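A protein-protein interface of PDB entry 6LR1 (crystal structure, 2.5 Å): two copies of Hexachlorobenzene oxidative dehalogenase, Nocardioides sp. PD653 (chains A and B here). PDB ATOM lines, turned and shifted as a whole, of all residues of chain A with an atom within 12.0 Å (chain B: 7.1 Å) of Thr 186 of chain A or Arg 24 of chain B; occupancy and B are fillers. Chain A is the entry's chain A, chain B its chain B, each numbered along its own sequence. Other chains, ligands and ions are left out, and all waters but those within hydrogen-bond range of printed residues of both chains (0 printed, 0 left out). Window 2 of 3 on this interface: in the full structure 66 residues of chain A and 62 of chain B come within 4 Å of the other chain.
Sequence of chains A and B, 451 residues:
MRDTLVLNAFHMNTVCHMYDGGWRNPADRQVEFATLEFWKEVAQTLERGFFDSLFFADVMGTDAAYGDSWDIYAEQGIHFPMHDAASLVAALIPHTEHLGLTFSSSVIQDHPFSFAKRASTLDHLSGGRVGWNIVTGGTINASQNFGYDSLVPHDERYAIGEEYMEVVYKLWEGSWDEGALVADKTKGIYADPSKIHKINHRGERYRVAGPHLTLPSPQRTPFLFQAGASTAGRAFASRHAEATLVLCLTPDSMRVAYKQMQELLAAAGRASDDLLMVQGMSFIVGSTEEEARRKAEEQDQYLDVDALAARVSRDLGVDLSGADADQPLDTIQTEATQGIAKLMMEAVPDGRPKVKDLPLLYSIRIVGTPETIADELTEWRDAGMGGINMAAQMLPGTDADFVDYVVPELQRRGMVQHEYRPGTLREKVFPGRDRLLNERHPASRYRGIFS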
ATOM      1  N   LEU A 181     -25.993  15.963 -25.062  1.00  0.00           N
ATOM      2  CA  LEU A 181     -25.978  16.513 -23.708  1.00  0.00           C
ATOM      3  C   LEU A 181     -24.658  17.254 -23.489  1.00  0.00           C
ATOM      4  O   LEU A 181     -23.579  16.663 -23.572  1.00  0.00           O
ATOM      5  CB  LEU A 181     -26.141  15.414 -22.650  1.00  0.00           C
ATOM      6  CG  LEU A 181     -26.094  15.802 -21.152  1.00  0.00           C
ATOM      7  CD1 LEU A 181     -27.061  16.919 -20.816  1.00  0.00           C
ATOM      8  CD2 LEU A 181     -26.408  14.578 -20.317  1.00  0.00           C
ATOM      9  N   VAL A 182     -24.746  18.546 -23.205  1.00  0.00           N
ATOM     10  CA  VAL A 182     -23.562  19.335 -22.985  1.00  0.00           C
ATOM     11  C   VAL A 182     -23.473  19.722 -21.526  1.00  0.00           C
ATOM     12  O   VAL A 182     -22.434  19.530 -20.894  1.00  0.00           O
ATOM     13  CB  VAL A 182     -23.541  20.569 -23.914  1.00  0.00           C
ATOM     14  CG1 VAL A 182     -22.422  21.530 -23.512  1.00  0.00           C
ATOM     15  CG2 VAL A 182     -23.357  20.123 -25.379  1.00  0.00           C
ATOM     16  N   ALA A 183     -24.536  20.344 -21.035  1.00  0.00           N
ATOM     17  CA  ALA A 183     -24.703  20.659 -19.627  1.00  0.00           C
ATOM     18  C   ALA A 183     -23.565  21.486 -19.067  1.00  0.00           C
ATOM     19  O   ALA A 183     -23.195  21.310 -17.927  1.00  0.00           O
ATOM     20  CB  ALA A 183     -24.903  19.374 -18.792  1.00  0.00           C
ATOM     21  N   ASP A 184     -23.072  22.431 -19.855  1.00  0.00           N
ATOM     22  CA  ASP A 184     -22.027  23.363 -19.427  1.00  0.00           C
ATOM     23  C   ASP A 184     -22.696  24.625 -18.892  1.00  0.00           C
ATOM     24  O   ASP A 184     -23.341  25.345 -19.634  1.00  0.00           O
ATOM     25  CB  ASP A 184     -21.123  23.691 -20.615  1.00  0.00           C
ATOM     26  CG  ASP A 184     -19.841  24.404 -20.223  1.00  0.00           C
ATOM     27  OD1 ASP A 184     -19.698  24.920 -19.088  1.00  0.00           O
ATOM     28  OD2 ASP A 184     -18.976  24.471 -21.113  1.00  0.00           O
ATOM     29  N   LYS A 185     -22.544  24.869 -17.596  1.00  0.00           N
ATOM     30  CA  LYS A 185     -23.192  26.002 -16.928  1.00  0.00           C
ATOM     31  C   LYS A 185     -22.517  27.340 -17.254  1.00  0.00           C
ATOM     32  O   LYS A 185     -23.201  28.359 -17.484  1.00  0.00           O
ATOM     33  CB  LYS A 185     -23.173  25.798 -15.416  1.00  0.00           C
ATOM     34  CG  LYS A 185     -23.967  24.593 -14.974  1.00  0.00           C
ATOM     35  CD  LYS A 185     -24.118  24.563 -13.461  1.00  0.00           C
ATOM     36  CE  LYS A 185     -24.991  23.400 -13.018  1.00  0.00           C
ATOM     37  NZ  LYS A 185     -25.383  23.515 -11.583  1.00  0.00           N
ATOM     38  N   THR A 186     -21.183  27.334 -17.243  1.00  0.00           N
ATOM     39  CA  THR A 186     -20.394  28.500 -17.615  1.00  0.00           C
ATOM     40  C   THR A 186     -20.675  28.950 -19.042  1.00  0.00           C
ATOM     41  O   THR A 186     -21.006  30.125 -19.245  1.00  0.00           O
ATOM     42  CB  THR A 186     -18.900  28.221 -17.510  1.00  0.00           C
ATOM     43  OG1 THR A 186     -18.654  27.472 -16.318  1.00  0.00           O
ATOM     44  CG2 THR A 186     -18.082  29.571 -17.531  1.00  0.00           C
ATOM     45  N   LYS A 187     -20.557  28.045 -20.025  1.00  0.00           N
ATOM     46  CA  LYS A 187     -20.856  28.421 -21.428  1.00  0.00           C
ATOM     47  C   LYS A 187     -22.371  28.537 -21.731  1.00  0.00           C
ATOM     48  O   LYS A 187     -22.751  29.013 -22.790  1.00  0.00           O
ATOM     49  CB  LYS A 187     -20.190  27.460 -22.421  1.00  0.00           C
ATOM     50  CG  LYS A 187     -19.824  28.125 -23.755  1.00  0.00           C
ATOM     51  CD  LYS A 187     -19.869  27.174 -24.954  1.00  0.00           C
ATOM     52  CE  LYS A 187     -18.704  26.185 -24.964  1.00  0.00           C
ATOM     53  NZ  LYS A 187     -19.049  24.967 -25.751  1.00  0.00           N
ATOM     54  N   GLY A 188     -23.239  28.052 -20.835  1.00  0.00           N
ATOM     55  CA  GLY A 188     -24.689  28.225 -20.985  1.00  0.00           C
ATOM     56  C   GLY A 188     -25.325  27.397 -22.079  1.00  0.00           C
ATOM     57  O   GLY A 188     -26.220  27.887 -22.755  1.00  0.00           O
ATOM     58  N   ILE A 189     -24.884  26.147 -22.247  1.00  0.00           N
ATOM     59  CA  ILE A 189     -25.460  25.208 -23.240  1.00  0.00           C
ATOM     60  C   ILE A 189     -25.837  23.890 -22.505  1.00  0.00           C
ATOM     61  O   ILE A 189     -24.967  23.136 -22.071  1.00  0.00           O
ATOM     62  CB  ILE A 189     -24.477  24.902 -24.410  1.00  0.00           C
ATOM     63  CG1 ILE A 189     -23.862  26.195 -25.006  1.00  0.00           C
ATOM     64  CG2 ILE A 189     -25.159  24.075 -25.500  1.00  0.00           C
ATOM     65  CD1 ILE A 189     -24.828  27.070 -25.787  1.00  0.00           C
ATOM     66  N   TYR A 190     -27.132  23.631 -22.358  1.00  0.00           N
ATOM     67  CA  TYR A 190     -27.588  22.427 -21.690  1.00  0.00           C
ATOM     68  C   TYR A 190     -27.576  21.276 -22.691  1.00  0.00           C
ATOM     69  O   TYR A 190     -26.890  20.296 -22.461  1.00  0.00           O
ATOM     70  CB  TYR A 190     -28.961  22.563 -20.990  1.00  0.00           C
ATOM     71  CG  TYR A 190     -29.306  21.237 -20.373  1.00  0.00           C
ATOM     72  CD1 TYR A 190     -28.710  20.830 -19.182  1.00  0.00           C
ATOM     73  CD2 TYR A 190     -30.152  20.331 -21.045  1.00  0.00           C
ATOM     74  CE1 TYR A 190     -28.950  19.563 -18.684  1.00  0.00           C
ATOM     75  CE2 TYR A 190     -30.397  19.082 -20.535  1.00  0.00           C
ATOM     76  CZ  TYR A 190     -29.773  18.701 -19.369  1.00  0.00           C
ATOM     77  OH  TYR A 190     -30.034  17.457 -18.893  1.00  0.00           O
ATOM     78  N   ALA A 191     -28.311  21.383 -23.785  1.00  0.00           N
ATOM     79  CA  ALA A 191     -28.225  20.397 -24.869  1.00  0.00           C
ATOM     80  C   ALA A 191     -27.974  21.085 -26.211  1.00  0.00           C
ATOM     81  O   ALA A 191     -28.410  22.213 -26.407  1.00  0.00           O
ATOM     82  CB  ALA A 191     -29.495  19.574 -24.928  1.00  0.00           C
ATOM     83  N   VAL B  15     -34.939  19.612 -16.268  1.00  0.00           N
ATOM     84  CA  VAL B  15     -33.795  20.409 -15.824  1.00  0.00           C
ATOM     85  C   VAL B  15     -34.127  21.838 -15.332  1.00  0.00           C
ATOM     86  O   VAL B  15     -33.415  22.336 -14.452  1.00  0.00           O
ATOM     87  CB  VAL B  15     -32.658  20.408 -16.899  1.00  0.00           C
ATOM     88  CG1 VAL B  15     -33.057  21.133 -18.153  1.00  0.00           C
ATOM     89  CG2 VAL B  15     -31.365  20.972 -16.323  1.00  0.00           C
ATOM     90  N   CYS B  16     -35.185  22.484 -15.850  1.00  0.00           N
ATOM     91  CA  CYS B  16     -35.480  23.879 -15.449  1.00  0.00           C
ATOM     92  C   CYS B  16     -36.950  24.243 -15.531  1.00  0.00           C
ATOM     93  O   CYS B  16     -37.363  25.007 -16.395  1.00  0.00           O
ATOM     94  CB  CYS B  16     -34.668  24.855 -16.277  1.00  0.00           C
ATOM     95  SG  CYS B  16     -34.363  26.426 -15.453  1.00  0.00           S
ATOM     96  N   GLY B  21     -33.244  29.642 -17.115  1.00  0.00           N
ATOM     97  CA  GLY B  21     -31.791  29.897 -16.927  1.00  0.00           C
ATOM     98  C   GLY B  21     -31.250  29.423 -15.572  1.00  0.00           C
ATOM     99  O   GLY B  21     -30.008  29.328 -15.397  1.00  0.00           O
ATOM    100  N   GLY B  22     -32.153  29.124 -14.621  1.00  0.00           N
ATOM    101  CA  GLY B  22     -31.775  28.836 -13.239  1.00  0.00           C
ATOM    102  C   GLY B  22     -30.868  27.610 -13.089  1.00  0.00           C
ATOM    103  O   GLY B  22     -30.117  27.484 -12.097  1.00  0.00           O
ATOM    104  N   TRP B  23     -30.935  26.703 -14.062  1.00  0.00           N
ATOM    105  CA  TRP B  23     -30.046  25.534 -14.054  1.00  0.00           C
ATOM    106  C   TRP B  23     -28.564  25.892 -14.064  1.00  0.00           C
ATOM    107  O   TRP B  23     -27.741  25.130 -13.603  1.00  0.00           O
ATOM    108  CB  TRP B  23     -30.367  24.590 -15.220  1.00  0.00           C
ATOM    109  CG  TRP B  23     -30.003  25.155 -16.543  1.00  0.00           C
ATOM    110  CD1 TRP B  23     -30.742  25.999 -17.294  1.00  0.00           C
ATOM    111  CD2 TRP B  23     -28.796  24.915 -17.260  1.00  0.00           C
ATOM    112  NE1 TRP B  23     -30.081  26.299 -18.455  1.00  0.00           N
ATOM    113  CE2 TRP B  23     -28.876  25.653 -18.459  1.00  0.00           C
ATOM    114  CE3 TRP B  23     -27.662  24.138 -17.008  1.00  0.00           C
ATOM    115  CZ2 TRP B  23     -27.849  25.666 -19.403  1.00  0.00           C
ATOM    116  CZ3 TRP B  23     -26.652  24.137 -17.920  1.00  0.00           C
ATOM    117  CH2 TRP B  23     -26.743  24.901 -19.124  1.00  0.00           C
ATOM    118  N   ARG B  24     -28.230  27.057 -14.583  1.00  0.00           N
ATOM    119  CA  ARG B  24     -26.852  27.468 -14.631  1.00  0.00           C
ATOM    120  C   ARG B  24     -26.254  27.828 -13.284  1.00  0.00           C
ATOM    121  O   ARG B  24     -25.040  27.864 -13.168  1.00  0.00           O
ATOM    122  CB  ARG B  24     -26.672  28.628 -15.582  1.00  0.00           C
ATOM    123  CG  ARG B  24     -27.056  28.231 -16.981  1.00  0.00           C
ATOM    124  CD  ARG B  24     -26.948  29.419 -17.880  1.00  0.00           C
ATOM    125  NE  ARG B  24     -25.560  29.814 -18.077  1.00  0.00           N
ATOM    126  CZ  ARG B  24     -25.197  30.846 -18.834  1.00  0.00           C
ATOM    127  NH1 ARG B  24     -23.905  31.127 -18.977  1.00  0.00           N
ATOM    128  NH2 ARG B  24     -26.112  31.585 -19.460  1.00  0.00           N
ATOM    129  N   ASN B  25     -27.074  28.115 -12.282  1.00  0.00           N
ATOM    130  CA  ASN B  25     -26.562  28.456 -10.950  1.00  0.00           C
ATOM    131  C   ASN B  25     -25.638  27.285 -10.469  1.00  0.00           C
ATOM    132  O   ASN B  25     -26.092  26.165 -10.349  1.00  0.00           O
ATOM    133  CB  ASN B  25     -27.758  28.715 -10.005  1.00  0.00           C
ATOM    134  CG  ASN B  25     -27.355  29.248  -8.635  1.00  0.00           C
ATOM    135  OD1 ASN B  25     -26.258  28.984  -8.141  1.00  0.00           O
ATOM    136  ND2 ASN B  25     -28.252  30.018  -8.016  1.00  0.00           N
ATOM    137  N   PRO B  26     -24.339  27.544 -10.226  1.00  0.00           N
ATOM    138  CA  PRO B  26     -23.405  26.545  -9.693  1.00  0.00           C
ATOM    139  C   PRO B  26     -23.901  25.857  -8.419  1.00  0.00           C
ATOM    140  O   PRO B  26     -23.505  24.715  -8.116  1.00  0.00           O
ATOM    141  CB  PRO B  26     -22.143  27.363  -9.351  1.00  0.00           C
ATOM    142  CG  PRO B  26     -22.261  28.637 -10.095  1.00  0.00           C
ATOM    143  CD  PRO B  26     -23.715  28.875 -10.361  1.00  0.00           C
ATOM    144  N   ALA B  27     -24.723  26.587  -7.667  1.00  0.00           N
ATOM    145  CA  ALA B  27     -25.258  26.129  -6.394  1.00  0.00           C
ATOM    146  C   ALA B  27     -26.489  25.200  -6.548  1.00  0.00           C
ATOM    147  O   ALA B  27     -26.936  24.556  -5.591  1.00  0.00           O
ATOM    148  CB  ALA B  27     -25.609  27.359  -5.522  1.00  0.00           C
ATOM    149  N   ASP B  28     -27.033  25.151  -7.754  1.00  0.00           N
ATOM    150  CA  ASP B  28     -28.237  24.384  -8.020  1.00  0.00           C
ATOM    151  C   ASP B  28     -27.869  23.003  -8.559  1.00  0.00           C
ATOM    152  O   ASP B  28     -26.810  22.852  -9.164  1.00  0.00           O
ATOM    153  CB  ASP B  28     -29.092  25.166  -9.016  1.00  0.00           C
ATOM    154  CG  ASP B  28     -30.299  24.422  -9.444  1.00  0.00           C
ATOM    155  OD1 ASP B  28     -31.280  24.388  -8.659  1.00  0.00           O
ATOM    156  OD2 ASP B  28     -30.236  23.854 -10.558  1.00  0.00           O
ATOM    157  N   GLN B  30     -30.477  20.866 -10.379  1.00  0.00           N
ATOM    158  CA  GLN B  30     -31.471  20.328 -11.308  1.00  0.00           C
ATOM    159  C   GLN B  30     -30.916  19.577 -12.548  1.00  0.00           C
ATOM    160  O   GLN B  30     -31.649  18.766 -13.168  1.00  0.00           O
ATOM    161  CB  GLN B  30     -32.412  21.446 -11.772  1.00  0.00           C
ATOM    162  CG  GLN B  30     -33.319  22.019 -10.683  1.00  0.00           C
ATOM    163  CD  GLN B  30     -34.130  23.179 -11.211  1.00  0.00           C
ATOM    164  OE1 GLN B  30     -33.627  24.281 -11.272  1.00  0.00           O
ATOM    165  NE2 GLN B  30     -35.379  22.938 -11.600  1.00  0.00           N
ATOM    166  N   VAL B  31     -29.650  19.826 -12.925  1.00  0.00           N
ATOM    167  CA  VAL B  31     -29.020  19.024 -13.973  1.00  0.00           C
ATOM    168  C   VAL B  31     -29.020  17.520 -13.609  1.00  0.00           C
ATOM    169  O   VAL B  31     -28.792  16.672 -14.471  1.00  0.00           O
ATOM    170  CB  VAL B  31     -27.590  19.487 -14.342  1.00  0.00           C
ATOM    171  CG1 VAL B  31     -27.645  20.828 -15.066  1.00  0.00           C
ATOM    172  CG2 VAL B  31     -26.683  19.574 -13.123  1.00  0.00           C
ATOM    173  N   GLU B  75     -30.661  24.840 -25.795  1.00  0.00           N
ATOM    174  CA  GLU B  75     -29.515  25.468 -25.064  1.00  0.00           C
ATOM    175  C   GLU B  75     -29.820  25.872 -23.617  1.00  0.00           C
ATOM    176  O   GLU B  75     -28.927  25.848 -22.749  1.00  0.00           O
ATOM    177  CB  GLU B  75     -29.004  26.686 -25.810  1.00  0.00           C
ATOM    178  CG  GLU B  75     -28.228  26.354 -27.079  1.00  0.00           C
ATOM    179  CD  GLU B  75     -28.188  27.487 -28.086  1.00  0.00           C
ATOM    180  OE1 GLU B  75     -28.750  28.550 -27.800  1.00  0.00           O
ATOM    181  OE2 GLU B  75     -27.590  27.315 -29.170  1.00  0.00           O
ATOM    182  N   GLN B  76     -31.067  26.254 -23.355  1.00  0.00           N
ATOM    183  CA  GLN B  76     -31.463  26.647 -22.016  1.00  0.00           C
ATOM    184  C   GLN B  76     -32.353  25.634 -21.299  1.00  0.00           C
ATOM    185  O   GLN B  76     -32.789  25.875 -20.186  1.00  0.00           O
ATOM    186  CB  GLN B  76     -32.115  28.046 -22.042  1.00  0.00           C
ATOM    187  CG  GLN B  76     -31.202  29.170 -22.526  1.00  0.00           C
ATOM    188  CD  GLN B  76     -29.830  29.099 -21.907  1.00  0.00           C
ATOM    189  OE1 GLN B  76     -29.677  28.996 -20.682  1.00  0.00           O
ATOM    190  NE2 GLN B  76     -28.822  29.095 -22.755  1.00  0.00           N
ATOM    191  N   GLN B 301     -28.957  36.612 -10.816  1.00  0.00           N
ATOM    192  CA  GLN B 301     -27.888  36.553 -11.825  1.00  0.00           C
ATOM    193  C   GLN B 301     -28.166  35.506 -12.882  1.00  0.00           C
ATOM    194  O   GLN B 301     -27.838  35.715 -14.020  1.00  0.00           O
ATOM    195  CB  GLN B 301     -26.545  36.171 -11.199  1.00  0.00           C
ATOM    196  CG  GLN B 301     -25.888  37.229 -10.324  1.00  0.00           C
ATOM    197  CD  GLN B 301     -24.648  36.677  -9.607  1.00  0.00           C
ATOM    198  OE1 GLN B 301     -24.732  36.065  -8.524  1.00  0.00           O
ATOM    199  NE2 GLN B 301     -23.488  36.885 -10.220  1.00  0.00           N
ATOM    200  N   TYR B 302     -28.731  34.362 -12.492  1.00  0.00           N
ATOM    201  CA  TYR B 302     -28.956  33.253 -13.418  1.00  0.00           C
ATOM    202  C   TYR B 302     -30.301  33.293 -14.120  1.00  0.00           C
ATOM    203  O   TYR B 302     -30.582  32.423 -14.931  1.00  0.00           O
ATOM    204  CB  TYR B 302     -28.718  31.911 -12.688  1.00  0.00           C
ATOM    205  CG  TYR B 302     -27.303  31.860 -12.168  1.00  0.00           C
ATOM    206  CD1 TYR B 302     -26.239  31.592 -13.030  1.00  0.00           C
ATOM    207  CD2 TYR B 302     -27.011  32.172 -10.833  1.00  0.00           C
ATOM    208  CE1 TYR B 302     -24.910  31.611 -12.573  1.00  0.00           C
ATOM    209  CE2 TYR B 302     -25.681  32.190 -10.363  1.00  0.00           C
ATOM    210  CZ  TYR B 302     -24.635  31.924 -11.234  1.00  0.00           C
ATOM    211  OH  TYR B 302     -23.323  31.937 -10.786  1.00  0.00           O
ATOM    212  N   ASP B 304     -32.422  34.173 -16.965  1.00  0.00           N
ATOM    213  CA  ASP B 304     -32.139  34.422 -18.393  1.00  0.00           C
ATOM    214  C   ASP B 304     -33.445  34.918 -18.984  1.00  0.00           C
ATOM    215  O   ASP B 304     -34.389  34.148 -19.164  1.00  0.00           O
ATOM    216  CB  ASP B 304     -31.666  33.101 -19.050  1.00  0.00           C
ATOM    217  CG  ASP B 304     -31.406  33.197 -20.561  1.00  0.00           C
ATOM    218  OD1 ASP B 304     -32.151  33.878 -21.283  1.00  0.00           O
ATOM    219  OD2 ASP B 304     -30.478  32.502 -21.042  1.00  0.00           O
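Of chain B, only Arg 24 (3.1 Å) comes within 4 Å of Thr 186 of chain A. No residue of chain A comes within 4 Å of Gly 21 of chain B. No residue of chain A comes within 4 Å of Gly 22 of chain B. No residue of chain A comes within 4 Å of Pro 26 of chain B. Of the printed residues of chain A, Gln 76 of chain B touches Gly 188. Tyr 302 of chain B touches none of the printed residues of chain A. Of the printed residues of chain B, Gly 188 of chain A touches Arg 24, Glu 75 and Gln 76. Of the printed residues of chain B, Ala 191 of chain A touches Glu 75. Printed residues of chain A within 4 Å of Val 15 of chain B: Tyr 190 (3.7 Å). Val 31 of chain B touches none of the printed residues of chain A. Gln 30 of chain B touches none of the printed residues of chain A. The nearest residue of chain A that does not touch Arg 24 of chain B is Lys 187 of chain A (4.1 Å).
NZ of Lys 185 of chain A sits at hydrogen-bond distance from O of Asp 28 of chain B (2.9 Å). O of Gly 188 of chain A lies within hydrogen-bond range of NE2 of Gln 76 of chain B. The backbone carbonyl oxygen of Thr 186 of chain A sits at hydrogen-bond distance from the guanidinium group of Arg 24 of chain B. O of Gly 188 of chain A sits close to O of Glu 75 of chain B (3.4 Å). The side-chain amino group (NZ) of Lys 185 of chain A sits close to the backbone carbonyl oxygen (O) of Trp 23 of chain B (3.5 Å). The side-chain amino group (NZ) of Lys 185 of chain A is in hydrogen-bond range of the backbone carbonyl oxygen (O) of Asn 25 of chain B, 3.0 Å away. O of Glu 75 of chain B sits at hydrogen-bond distance from N of Tyr 190 of chain A (2.9 Å). The backbone carbonyl oxygen (O) of Lys 185 of chain A is in hydrogen-bond range of the guanidinium group (NE) of Arg 24 of chain B, 2.8 Å away.
Among the printed residues, merely in contact across the chains: Gly 188 of chain A with Arg 24 of chain B, Asp 184 of chain A with Trp 23 of chain B, Tyr 190 of chain A with Trp 23 of chain B, Ala 191 of chain A with Glu 75 of chain B, Ile 189 of chain A with Glu 75 of chain B, Ile 189 of chain A with Trp 23 of chain B and Tyr 190 of chain A with Val 15 of chain B.
No position is printed for both chains.
Of the 11 printed residues of chain A, 7 touch a printed residue of chain B. Printed residues of chain A that touch a printed residue of chain B: Asp 184, Lys 185, Thr 186, Gly 188, Ile 189, Tyr 190 and Ala 191. Hydrophobic or aromatic side chains of chain B within 4 Å of the printed part of chain A: Val 15 and Trp 23. Among the printed residues, 15 pairs touch across the chains.
N of Ala 183 of chain A sits at hydrogen-bond distance from O of Ile 189 of chain A, 3.0 Å away. N of Val 182 of chain A is in hydrogen-bond range of O of Tyr 190 of chain A (2.9 Å). OD1 of Asp 184 of chain A lies within hydrogen-bond range of N of Lys 187 of chain A, at 3.4 Å. The backbone NH (N) of Thr 186 of chain A lies within hydrogen-bond range of the side-chain carboxylate (OD1) of Asp 184 of chain A (3.4 Å). The side-chain amide oxygen (OD1) of Asn 25 of chain B lies within hydrogen-bond range of the backbone NH (N) of Ala 27 of chain B, at 2.9 Å. NE1 of Trp 23 of chain B sits at hydrogen-bond distance from O of Gln 76 of chain B, at 3.2 Å.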
